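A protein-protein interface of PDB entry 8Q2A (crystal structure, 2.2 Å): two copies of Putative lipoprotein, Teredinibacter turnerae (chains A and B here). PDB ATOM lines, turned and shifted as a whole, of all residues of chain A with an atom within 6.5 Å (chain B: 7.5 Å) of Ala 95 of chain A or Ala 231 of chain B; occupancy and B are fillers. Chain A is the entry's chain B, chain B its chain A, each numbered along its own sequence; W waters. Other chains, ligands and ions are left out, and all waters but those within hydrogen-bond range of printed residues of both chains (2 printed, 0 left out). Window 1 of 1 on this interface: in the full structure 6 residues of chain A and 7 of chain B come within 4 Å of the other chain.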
ATOM      1  N   ASN A  93     -20.746  29.607 -10.383  1.00  0.00           N
ATOM      2  CA  ASN A  93     -19.869  28.469 -10.642  1.00  0.00           C
ATOM      3  C   ASN A  93     -19.546  27.705  -9.349  1.00  0.00           C
ATOM      4  O   ASN A  93     -18.391  27.551  -8.951  1.00  0.00           O
ATOM      5  CB  ASN A  93     -18.574  28.915 -11.299  1.00  0.00           C
ATOM      6  CG  ASN A  93     -17.835  27.736 -11.857  1.00  0.00           C
ATOM      7  OD1 ASN A  93     -18.440  26.736 -12.214  1.00  0.00           O
ATOM      8  ND2 ASN A  93     -16.515  27.801 -11.807  1.00  0.00           N
ATOM      9  N   GLU A  94     -20.564  27.134  -8.740  1.00  0.00           N
ATOM     10  CA  GLU A  94     -20.338  26.531  -7.433  1.00  0.00           C
ATOM     11  C   GLU A  94     -21.323  25.394  -7.222  1.00  0.00           C
ATOM     12  O   GLU A  94     -22.480  25.551  -7.454  1.00  0.00           O
ATOM     13  CB  GLU A  94     -20.563  27.616  -6.383  1.00  0.00           C
ATOM     14  CG  GLU A  94     -20.528  27.170  -4.960  1.00  0.00           C
ATOM     15  CD  GLU A  94     -20.293  28.400  -4.095  1.00  0.00           C
ATOM     16  OE1 GLU A  94     -21.028  28.531  -3.087  1.00  0.00           O
ATOM     17  OE2 GLU A  94     -19.425  29.266  -4.509  1.00  0.00           O
ATOM     18  N   ALA A  95     -20.836  24.258  -6.761  1.00  0.00           N
ATOM     19  CA  ALA A  95     -21.616  23.080  -6.423  1.00  0.00           C
ATOM     20  C   ALA A  95     -22.623  23.358  -5.317  1.00  0.00           C
ATOM     21  O   ALA A  95     -22.352  24.136  -4.442  1.00  0.00           O
ATOM     22  CB  ALA A  95     -20.680  21.968  -6.067  1.00  0.00           C
ATOM     23  N   ASN A  96     -23.852  22.834  -5.513  1.00  0.00           N
ATOM     24  CA  ASN A  96     -24.845  22.609  -4.480  1.00  0.00           C
ATOM     25  C   ASN A  96     -25.516  23.878  -3.968  1.00  0.00           C
ATOM     26  O   ASN A  96     -26.154  23.848  -2.933  1.00  0.00           O
ATOM     27  CB  ASN A  96     -24.258  21.852  -3.262  1.00  0.00           C
ATOM     28  CG  ASN A  96     -25.391  21.294  -2.429  1.00  0.00           C
ATOM     29  OD1 ASN A  96     -26.359  20.803  -3.028  1.00  0.00           O
ATOM     30  ND2 ASN A  96     -25.333  21.457  -1.110  1.00  0.00           N
ATOM     31  N   ASP A  97     -25.380  25.009  -4.654  1.00  0.00           N
ATOM     32  CA  ASP A  97     -26.016  26.249  -4.201  1.00  0.00           C
ATOM     33  C   ASP A  97     -27.507  26.176  -4.509  1.00  0.00           C
ATOM     34  O   ASP A  97     -27.912  25.606  -5.501  1.00  0.00           O
ATOM     35  CB  ASP A  97     -25.351  27.460  -4.857  1.00  0.00           C
ATOM     36  CG  ASP A  97     -26.091  28.779  -4.655  1.00  0.00           C
ATOM     37  OD1 ASP A  97     -26.117  29.260  -3.504  1.00  0.00           O
ATOM     38  OD2 ASP A  97     -26.691  29.312  -5.695  1.00  0.00           O
ATOM     39  N   GLY A 123     -26.011  28.016  -8.290  1.00  0.00           N
ATOM     40  CA  GLY A 123     -24.593  28.015  -8.583  1.00  0.00           C
ATOM     41  C   GLY A 123     -24.256  28.638  -9.933  1.00  0.00           C
ATOM     42  O   GLY A 123     -23.165  28.429 -10.414  1.00  0.00           O
ATOM     43  N   TRP A 142     -26.937  25.645 -14.794  1.00  0.00           N
ATOM     44  CA  TRP A 142     -26.636  25.672 -13.374  1.00  0.00           C
ATOM     45  C   TRP A 142     -25.256  25.052 -13.045  1.00  0.00           C
ATOM     46  O   TRP A 142     -24.657  24.296 -13.825  1.00  0.00           O
ATOM     47  CB  TRP A 142     -27.756  24.977 -12.611  1.00  0.00           C
ATOM     48  CG  TRP A 142     -29.090  25.660 -12.779  1.00  0.00           C
ATOM     49  CD1 TRP A 142     -29.309  26.873 -13.331  1.00  0.00           C
ATOM     50  CD2 TRP A 142     -30.359  25.171 -12.358  1.00  0.00           C
ATOM     51  NE1 TRP A 142     -30.626  27.161 -13.269  1.00  0.00           N
ATOM     52  CE2 TRP A 142     -31.297  26.142 -12.680  1.00  0.00           C
ATOM     53  CE3 TRP A 142     -30.790  24.018 -11.717  1.00  0.00           C
ATOM     54  CZ2 TRP A 142     -32.650  26.001 -12.444  1.00  0.00           C
ATOM     55  CZ3 TRP A 142     -32.150  23.820 -11.542  1.00  0.00           C
ATOM     56  CH2 TRP A 142     -33.073  24.799 -11.918  1.00  0.00           C
ATOM     57  N   TYR A 143     -24.707  25.482 -11.896  1.00  0.00           N
ATOM     58  CA  TYR A 143     -23.473  25.008 -11.355  1.00  0.00           C
ATOM     59  C   TYR A 143     -22.366  25.168 -12.374  1.00  0.00           C
ATOM     60  O   TYR A 143     -21.672  24.200 -12.739  1.00  0.00           O
ATOM     61  CB  TYR A 143     -23.653  23.540 -10.997  1.00  0.00           C
ATOM     62  CG  TYR A 143     -24.901  23.347 -10.183  1.00  0.00           C
ATOM     63  CD1 TYR A 143     -25.086  23.951  -8.922  1.00  0.00           C
ATOM     64  CD2 TYR A 143     -25.904  22.538 -10.716  1.00  0.00           C
ATOM     65  CE1 TYR A 143     -26.243  23.671  -8.195  1.00  0.00           C
ATOM     66  CE2 TYR A 143     -27.090  22.319 -10.019  1.00  0.00           C
ATOM     67  CZ  TYR A 143     -27.250  22.878  -8.783  1.00  0.00           C
ATOM     68  OH  TYR A 143     -28.439  22.436  -8.387  1.00  0.00           O
ATOM     69  N   SER A 144     -22.249  26.371 -12.884  1.00  0.00           N
ATOM     70  CA  SER A 144     -21.241  26.673 -13.871  1.00  0.00           C
ATOM     71  C   SER A 144     -21.223  28.191 -14.140  1.00  0.00           C
ATOM     72  O   SER A 144     -21.753  28.973 -13.346  1.00  0.00           O
ATOM     73  CB  SER A 144     -21.499  25.852 -15.137  1.00  0.00           C
ATOM     74  OG  SER A 144     -22.546  26.422 -15.869  1.00  0.00           O
ATOM     75  N   SER B   2     -23.490  16.525 -15.600  1.00  0.00           N
ATOM     76  CA  SER B   2     -23.237  17.810 -14.882  1.00  0.00           C
ATOM     77  C   SER B   2     -24.373  18.056 -13.902  1.00  0.00           C
ATOM     78  O   SER B   2     -25.435  17.447 -13.973  1.00  0.00           O
ATOM     79  CB  SER B   2     -22.785  18.974 -15.736  1.00  0.00           C
ATOM     80  OG  SER B   2     -23.816  19.589 -16.474  1.00  0.00           O
ATOM     81  N   GLY B   3     -24.007  18.816 -12.881  1.00  0.00           N
ATOM     82  CA  GLY B   3     -24.775  18.998 -11.675  1.00  0.00           C
ATOM     83  C   GLY B   3     -24.359  18.008 -10.611  1.00  0.00           C
ATOM     84  O   GLY B   3     -25.005  17.980  -9.533  1.00  0.00           O
ATOM     85  N   PHE B   4     -23.361  17.150 -10.898  1.00  0.00           N
ATOM     86  CA  PHE B   4     -23.017  16.060 -10.010  1.00  0.00           C
ATOM     87  C   PHE B   4     -22.501  16.634  -8.702  1.00  0.00           C
ATOM     88  O   PHE B   4     -21.588  17.444  -8.762  1.00  0.00           O
ATOM     89  CB  PHE B   4     -22.037  15.081 -10.639  1.00  0.00           C
ATOM     90  CG  PHE B   4     -21.437  14.126  -9.654  1.00  0.00           C
ATOM     91  CD1 PHE B   4     -22.236  13.311  -8.893  1.00  0.00           C
ATOM     92  CD2 PHE B   4     -20.072  14.147  -9.399  1.00  0.00           C
ATOM     93  CE1 PHE B   4     -21.700  12.445  -7.940  1.00  0.00           C
ATOM     94  CE2 PHE B   4     -19.533  13.310  -8.447  1.00  0.00           C
ATOM     95  CZ  PHE B   4     -20.350  12.421  -7.734  1.00  0.00           C
ATOM     96  N   PHE B   5     -23.147  16.256  -7.582  1.00  0.00           N
ATOM     97  CA  PHE B   5     -22.693  16.593  -6.248  1.00  0.00           C
ATOM     98  C   PHE B   5     -23.198  15.540  -5.264  1.00  0.00           C
ATOM     99  O   PHE B   5     -24.365  15.185  -5.283  1.00  0.00           O
ATOM    100  CB  PHE B   5     -23.210  17.970  -5.820  1.00  0.00           C
ATOM    101  CG  PHE B   5     -22.961  18.320  -4.380  1.00  0.00           C
ATOM    102  CD1 PHE B   5     -23.869  17.957  -3.410  1.00  0.00           C
ATOM    103  CD2 PHE B   5     -21.756  18.863  -3.991  1.00  0.00           C
ATOM    104  CE1 PHE B   5     -23.594  18.206  -2.063  1.00  0.00           C
ATOM    105  CE2 PHE B   5     -21.493  19.135  -2.667  1.00  0.00           C
ATOM    106  CZ  PHE B   5     -22.404  18.788  -1.691  1.00  0.00           C
ATOM    107  N   VAL B   6     -22.317  15.089  -4.369  1.00  0.00           N
ATOM    108  CA  VAL B   6     -22.625  14.130  -3.306  1.00  0.00           C
ATOM    109  C   VAL B   6     -21.806  14.468  -2.083  1.00  0.00           C
ATOM    110  O   VAL B   6     -20.657  14.837  -2.168  1.00  0.00           O
ATOM    111  CB  VAL B   6     -22.322  12.676  -3.711  1.00  0.00           C
ATOM    112  CG1 VAL B   6     -22.533  11.718  -2.550  1.00  0.00           C
ATOM    113  CG2 VAL B   6     -23.193  12.262  -4.885  1.00  0.00           C
ATOM    114  N   ARG B  78     -14.753  17.444 -15.142  1.00  0.00           N
ATOM    115  CA  ARG B  78     -13.930  17.843 -14.021  1.00  0.00           C
ATOM    116  C   ARG B  78     -14.347  17.108 -12.767  1.00  0.00           C
ATOM    117  O   ARG B  78     -15.473  16.719 -12.647  1.00  0.00           O
ATOM    118  CB  ARG B  78     -13.879  19.362 -13.883  1.00  0.00           C
ATOM    119  CG  ARG B  78     -15.127  20.211 -14.028  1.00  0.00           C
ATOM    120  CD  ARG B  78     -14.772  21.639 -14.480  1.00  0.00           C
ATOM    121  NE  ARG B  78     -15.918  22.510 -14.246  1.00  0.00           N
ATOM    122  CZ  ARG B  78     -15.930  23.728 -13.627  1.00  0.00           C
ATOM    123  NH1 ARG B  78     -14.811  24.441 -13.381  1.00  0.00           N
ATOM    124  NH2 ARG B  78     -17.130  24.239 -13.319  1.00  0.00           N
ATOM    125  N   VAL B  79     -13.437  16.969 -11.822  1.00  0.00           N
ATOM    126  CA  VAL B  79     -13.767  16.388 -10.535  1.00  0.00           C
ATOM    127  C   VAL B  79     -13.199  17.261  -9.441  1.00  0.00           C
ATOM    128  O   VAL B  79     -12.055  17.635  -9.487  1.00  0.00           O
ATOM    129  CB  VAL B  79     -13.243  14.938 -10.372  1.00  0.00           C
ATOM    130  CG1 VAL B  79     -13.507  14.386  -8.962  1.00  0.00           C
ATOM    131  CG2 VAL B  79     -13.922  13.995 -11.313  1.00  0.00           C
ATOM    132  N   TYR B  80     -14.009  17.506  -8.446  1.00  0.00           N
ATOM    133  CA  TYR B  80     -13.586  18.139  -7.219  1.00  0.00           C
ATOM    134  C   TYR B  80     -13.831  17.146  -6.112  1.00  0.00           C
ATOM    135  O   TYR B  80     -14.880  16.503  -6.085  1.00  0.00           O
ATOM    136  CB  TYR B  80     -14.370  19.435  -6.971  1.00  0.00           C
ATOM    137  CG  TYR B  80     -14.129  20.511  -8.020  1.00  0.00           C
ATOM    138  CD1 TYR B  80     -14.729  20.447  -9.260  1.00  0.00           C
ATOM    139  CD2 TYR B  80     -13.363  21.643  -7.725  1.00  0.00           C
ATOM    140  CE1 TYR B  80     -14.485  21.424 -10.220  1.00  0.00           C
ATOM    141  CE2 TYR B  80     -13.140  22.639  -8.660  1.00  0.00           C
ATOM    142  CZ  TYR B  80     -13.663  22.502  -9.941  1.00  0.00           C
ATOM    143  OH  TYR B  80     -13.463  23.469 -10.902  1.00  0.00           O
ATOM    144  N   LEU B  81     -12.866  17.033  -5.219  1.00  0.00           N
ATOM    145  CA  LEU B  81     -12.947  16.158  -4.064  1.00  0.00           C
ATOM    146  C   LEU B  81     -12.653  17.016  -2.876  1.00  0.00           C
ATOM    147  O   LEU B  81     -11.778  17.846  -2.976  1.00  0.00           O
ATOM    148  CB  LEU B  81     -11.919  15.013  -4.105  1.00  0.00           C
ATOM    149  CG  LEU B  81     -11.928  14.138  -5.342  1.00  0.00           C
ATOM    150  CD1 LEU B  81     -10.841  13.067  -5.247  1.00  0.00           C
ATOM    151  CD2 LEU B  81     -13.286  13.497  -5.404  1.00  0.00           C
ATOM    152  N   GLU B 159      -8.918  19.787  -7.074  1.00  0.00           N
ATOM    153  CA  GLU B 159      -9.643  20.220  -8.259  1.00  0.00           C
ATOM    154  C   GLU B 159      -8.928  19.581  -9.424  1.00  0.00           C
ATOM    155  O   GLU B 159      -7.732  19.748  -9.532  1.00  0.00           O
ATOM    156  CB  GLU B 159      -9.647  21.759  -8.306  1.00  0.00           C
ATOM    157  CG  GLU B 159      -9.938  22.425  -9.667  1.00  0.00           C
ATOM    158  CD  GLU B 159     -10.050  23.977  -9.689  1.00  0.00           C
ATOM    159  OE1 GLU B 159      -9.034  24.619  -9.237  1.00  0.00           O
ATOM    160  OE2 GLU B 159     -11.177  24.599 -10.159  1.00  0.00           O
ATOM    161  N   GLU B 227     -16.994  15.359   0.164  1.00  0.00           N
ATOM    162  CA  GLU B 227     -17.816  15.857  -0.924  1.00  0.00           C
ATOM    163  C   GLU B 227     -17.094  15.576  -2.234  1.00  0.00           C
ATOM    164  O   GLU B 227     -15.849  15.487  -2.329  1.00  0.00           O
ATOM    165  CB  GLU B 227     -18.120  17.367  -0.819  1.00  0.00           C
ATOM    166  CG  GLU B 227     -18.573  17.871   0.587  1.00  0.00           C
ATOM    167  CD  GLU B 227     -19.011  19.334   0.836  1.00  0.00           C
ATOM    168  OE1 GLU B 227     -19.109  20.156  -0.161  1.00  0.00           O
ATOM    169  OE2 GLU B 227     -19.233  19.723   2.091  1.00  0.00           O
ATOM    170  N   MET B 228     -17.911  15.356  -3.245  1.00  0.00           N
ATOM    171  CA  MET B 228     -17.437  15.149  -4.592  1.00  0.00           C
ATOM    172  C   MET B 228     -18.441  15.746  -5.572  1.00  0.00           C
ATOM    173  O   MET B 228     -19.636  15.838  -5.331  1.00  0.00           O
ATOM    174  CB  MET B 228     -17.223  13.666  -4.913  1.00  0.00           C
ATOM    175  CG  MET B 228     -18.328  12.765  -4.493  1.00  0.00           C
ATOM    176  SD  MET B 228     -17.815  11.031  -4.933  1.00  0.00           S
ATOM    177  CE  MET B 228     -16.972  10.550  -3.442  1.00  0.00           C
ATOM    178  N   SER B 229     -17.905  16.217  -6.690  1.00  0.00           N
ATOM    179  CA  SER B 229     -18.612  17.188  -7.468  1.00  0.00           C
ATOM    180  C   SER B 229     -17.959  17.365  -8.830  1.00  0.00           C
ATOM    181  O   SER B 229     -16.796  17.062  -8.944  1.00  0.00           O
ATOM    182  CB  SER B 229     -18.601  18.452  -6.714  1.00  0.00           C
ATOM    183  OG  SER B 229     -19.447  19.371  -7.335  1.00  0.00           O
ATOM    184  N   ASP B 230     -18.720  17.876  -9.826  1.00  0.00           N
ATOM    185  CA  ASP B 230     -18.117  18.363 -11.055  1.00  0.00           C
ATOM    186  C   ASP B 230     -18.273  19.864 -11.162  1.00  0.00           C
ATOM    187  O   ASP B 230     -18.168  20.429 -12.264  1.00  0.00           O
ATOM    188  CB  ASP B 230     -18.598  17.678 -12.330  1.00  0.00           C
ATOM    189  CG  ASP B 230     -20.018  17.960 -12.770  1.00  0.00           C
ATOM    190  OD1 ASP B 230     -20.860  18.124 -11.838  1.00  0.00           O
ATOM    191  OD2 ASP B 230     -20.262  17.868 -14.052  1.00  0.00           O
ATOM    192  N   ALA B 231     -18.556  20.506 -10.016  1.00  0.00           N
ATOM    193  CA  ALA B 231     -18.424  21.957  -9.974  1.00  0.00           C
ATOM    194  C   ALA B 231     -17.683  22.346  -8.712  1.00  0.00           C
ATOM    195  O   ALA B 231     -17.690  21.577  -7.731  1.00  0.00           O
ATOM    196  CB  ALA B 231     -19.788  22.570 -10.007  1.00  0.00           C
ATOM    197  N   PRO B 232     -17.090  23.550  -8.655  1.00  0.00           N
ATOM    198  CA  PRO B 232     -16.240  23.918  -7.524  1.00  0.00           C
ATOM    199  C   PRO B 232     -16.841  23.698  -6.140  1.00  0.00           C
ATOM    200  O   PRO B 232     -17.998  23.961  -5.896  1.00  0.00           O
ATOM    201  CB  PRO B 232     -15.741  25.368  -7.811  1.00  0.00           C
ATOM    202  CG  PRO B 232     -15.924  25.540  -9.305  1.00  0.00           C
ATOM    203  CD  PRO B 232     -16.951  24.496  -9.762  1.00  0.00           C
ATOM    204  N   LEU B 233     -15.989  23.216  -5.239  1.00  0.00           N
ATOM    205  CA  LEU B 233     -16.235  23.132  -3.802  1.00  0.00           C
ATOM    206  C   LEU B 233     -15.238  24.053  -3.094  1.00  0.00           C
ATOM    207  O   LEU B 233     -14.131  24.216  -3.553  1.00  0.00           O
ATOM    208  CB  LEU B 233     -15.955  21.675  -3.422  1.00  0.00           C
ATOM    209  CG  LEU B 233     -16.826  20.633  -4.108  1.00  0.00           C
ATOM    210  CD1 LEU B 233     -16.278  19.248  -3.886  1.00  0.00           C
ATOM    211  CD2 LEU B 233     -18.260  20.774  -3.631  1.00  0.00           C
ATOM    212  N   THR B 234     -15.564  24.597  -1.954  1.00  0.00           N
ATOM    213  CA  THR B 234     -14.629  25.466  -1.229  1.00  0.00           C
ATOM    214  C   THR B 234     -14.797  25.236   0.278  1.00  0.00           C
ATOM    215  O   THR B 234     -15.831  24.745   0.747  1.00  0.00           O
ATOM    216  CB  THR B 234     -14.745  26.979  -1.615  1.00  0.00           C
ATOM    217  OG1 THR B 234     -15.934  27.521  -1.036  1.00  0.00           O
ATOM    218  CG2 THR B 234     -14.741  27.328  -3.105  1.00  0.00           C
HETATM  219  O   HOH W   1     -19.655  22.704 -13.117  1.00  0.00           O
HETATM  220  O   HOH W   2     -24.470  20.653  -7.773  1.00  0.00           O
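NH2 of Arg 78 of chain B lies within hydrogen-bond range of OD1 of Asn 93 of chain A, at 3.0 Å. The backbone NH (N) of Ala 95 of chain A is in hydrogen-bond range of the backbone carbonyl oxygen (O) of Pro 232 of chain B, at 3.0 Å.
The side-chain carboxylate of Asp 230 of chain B lies within hydrogen-bond range of the backbone NH of Gly 3 of chain B. O of Phe 4 of chain B is in hydrogen-bond range of OG of Ser 229 of chain B (3.2 Å). NH1 of Arg 78 of chain B sits at hydrogen-bond distance from OH of Tyr 80 of chain B (3.0 Å). The side-chain hydroxyl (OG) of Ser 229 of chain B is in hydrogen-bond range of the backbone carbonyl oxygen (O) of Ala 231 of chain B. N of Asn 93 of chain A sits at hydrogen-bond distance from O of Gly 123 of chain A (2.7 Å). The backbone NH of Glu 94 of chain A sits at hydrogen-bond distance from the backbone carbonyl oxygen of Gly 123 of chain A (3.4 Å).
CG of Pro 232 of chain B touches O of Asn 93 of chain A (3.2 Å). CA of Glu 94 of chain A touches O of Pro 232 of chain B, 3.8 Å away. Phe 5 of chain B touches Ala 95 of chain A. Ala 95 of chain A touches Ser 229 of chain B. Ala 95 of chain A touches Ala 231 of chain B (CB to O, 3.4 Å). Leu 233 of chain B touches Ala 95 of chain A. CG of Asn 96 of chain A touches CE1 of Phe 5 of chain B (3.6 Å). Tyr 143 of chain A touches Gly 3 of chain B. Tyr 143 of chain A touches Ala 231 of chain B.
Of the printed residues of chain B, Asn 93 of chain A touches Arg 78 and Pro 232. Of chain B, only Phe 5, Ser 229, Ala 231, Pro 232 and Leu 233 come within 4 Å of Ala 95 of chain A. Printed residues of chain B within 4 Å of Asn 96 of chain A: Phe 5 (3.6 Å). Of the printed residues of chain A, Gly 3 of chain B touches Tyr 143. Printed residues of chain A within 4 Å of Phe 5 of chain B: Ala 95 and Asn 96. Ala 231 of chain B touches just these residues of chain A: Ala 95 (3.4 Å) and Tyr 143 (3.7 Å). Of the printed residues of chain A, Pro 232 of chain B touches Asn 93 (3.2 Å), Glu 94 (3.8 Å) and Ala 95 (3.0 Å). The nearest residue of chain A that does not touch Ala 231 of chain B is Glu 94 of chain A (4.3 Å). The nearest printed residue of chain A that does not touch Arg 78 of chain B is Tyr 143 of chain A (4.6 Å).
Printed residues of chain A that touch a printed residue of chain B: Asn 93, Glu 94, Ala 95, Asn 96 and Tyr 143. Hydrophobic or aromatic side chains of chain B that line the printed part of chain A: Phe 5, Ala 231, Pro 232 and Leu 233. Among the printed residues, 11 pairs touch across the chains. Among the printed residues, no Asp or Glu carboxylate lies within 4 Å of a Lys or Arg side-chain nitrogen of the other chain.
No position is printed for both chains.
Water W1 lies within hydrogen-bond range of the backbone carbonyl oxygen of Tyr 143 of chain A (2.5 Å), the backbone carbonyl oxygen of Asp 230 of chain B (2.8 Å) and the guanidinium group of Arg 78 of chain B (3.0 Å). Water W2 bridges the backbone NH (N) of Asn 96 of chain A (3.2 Å) and the backbone carbonyl oxygen (O) of Gly 3 of chain B (3.2 Å).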
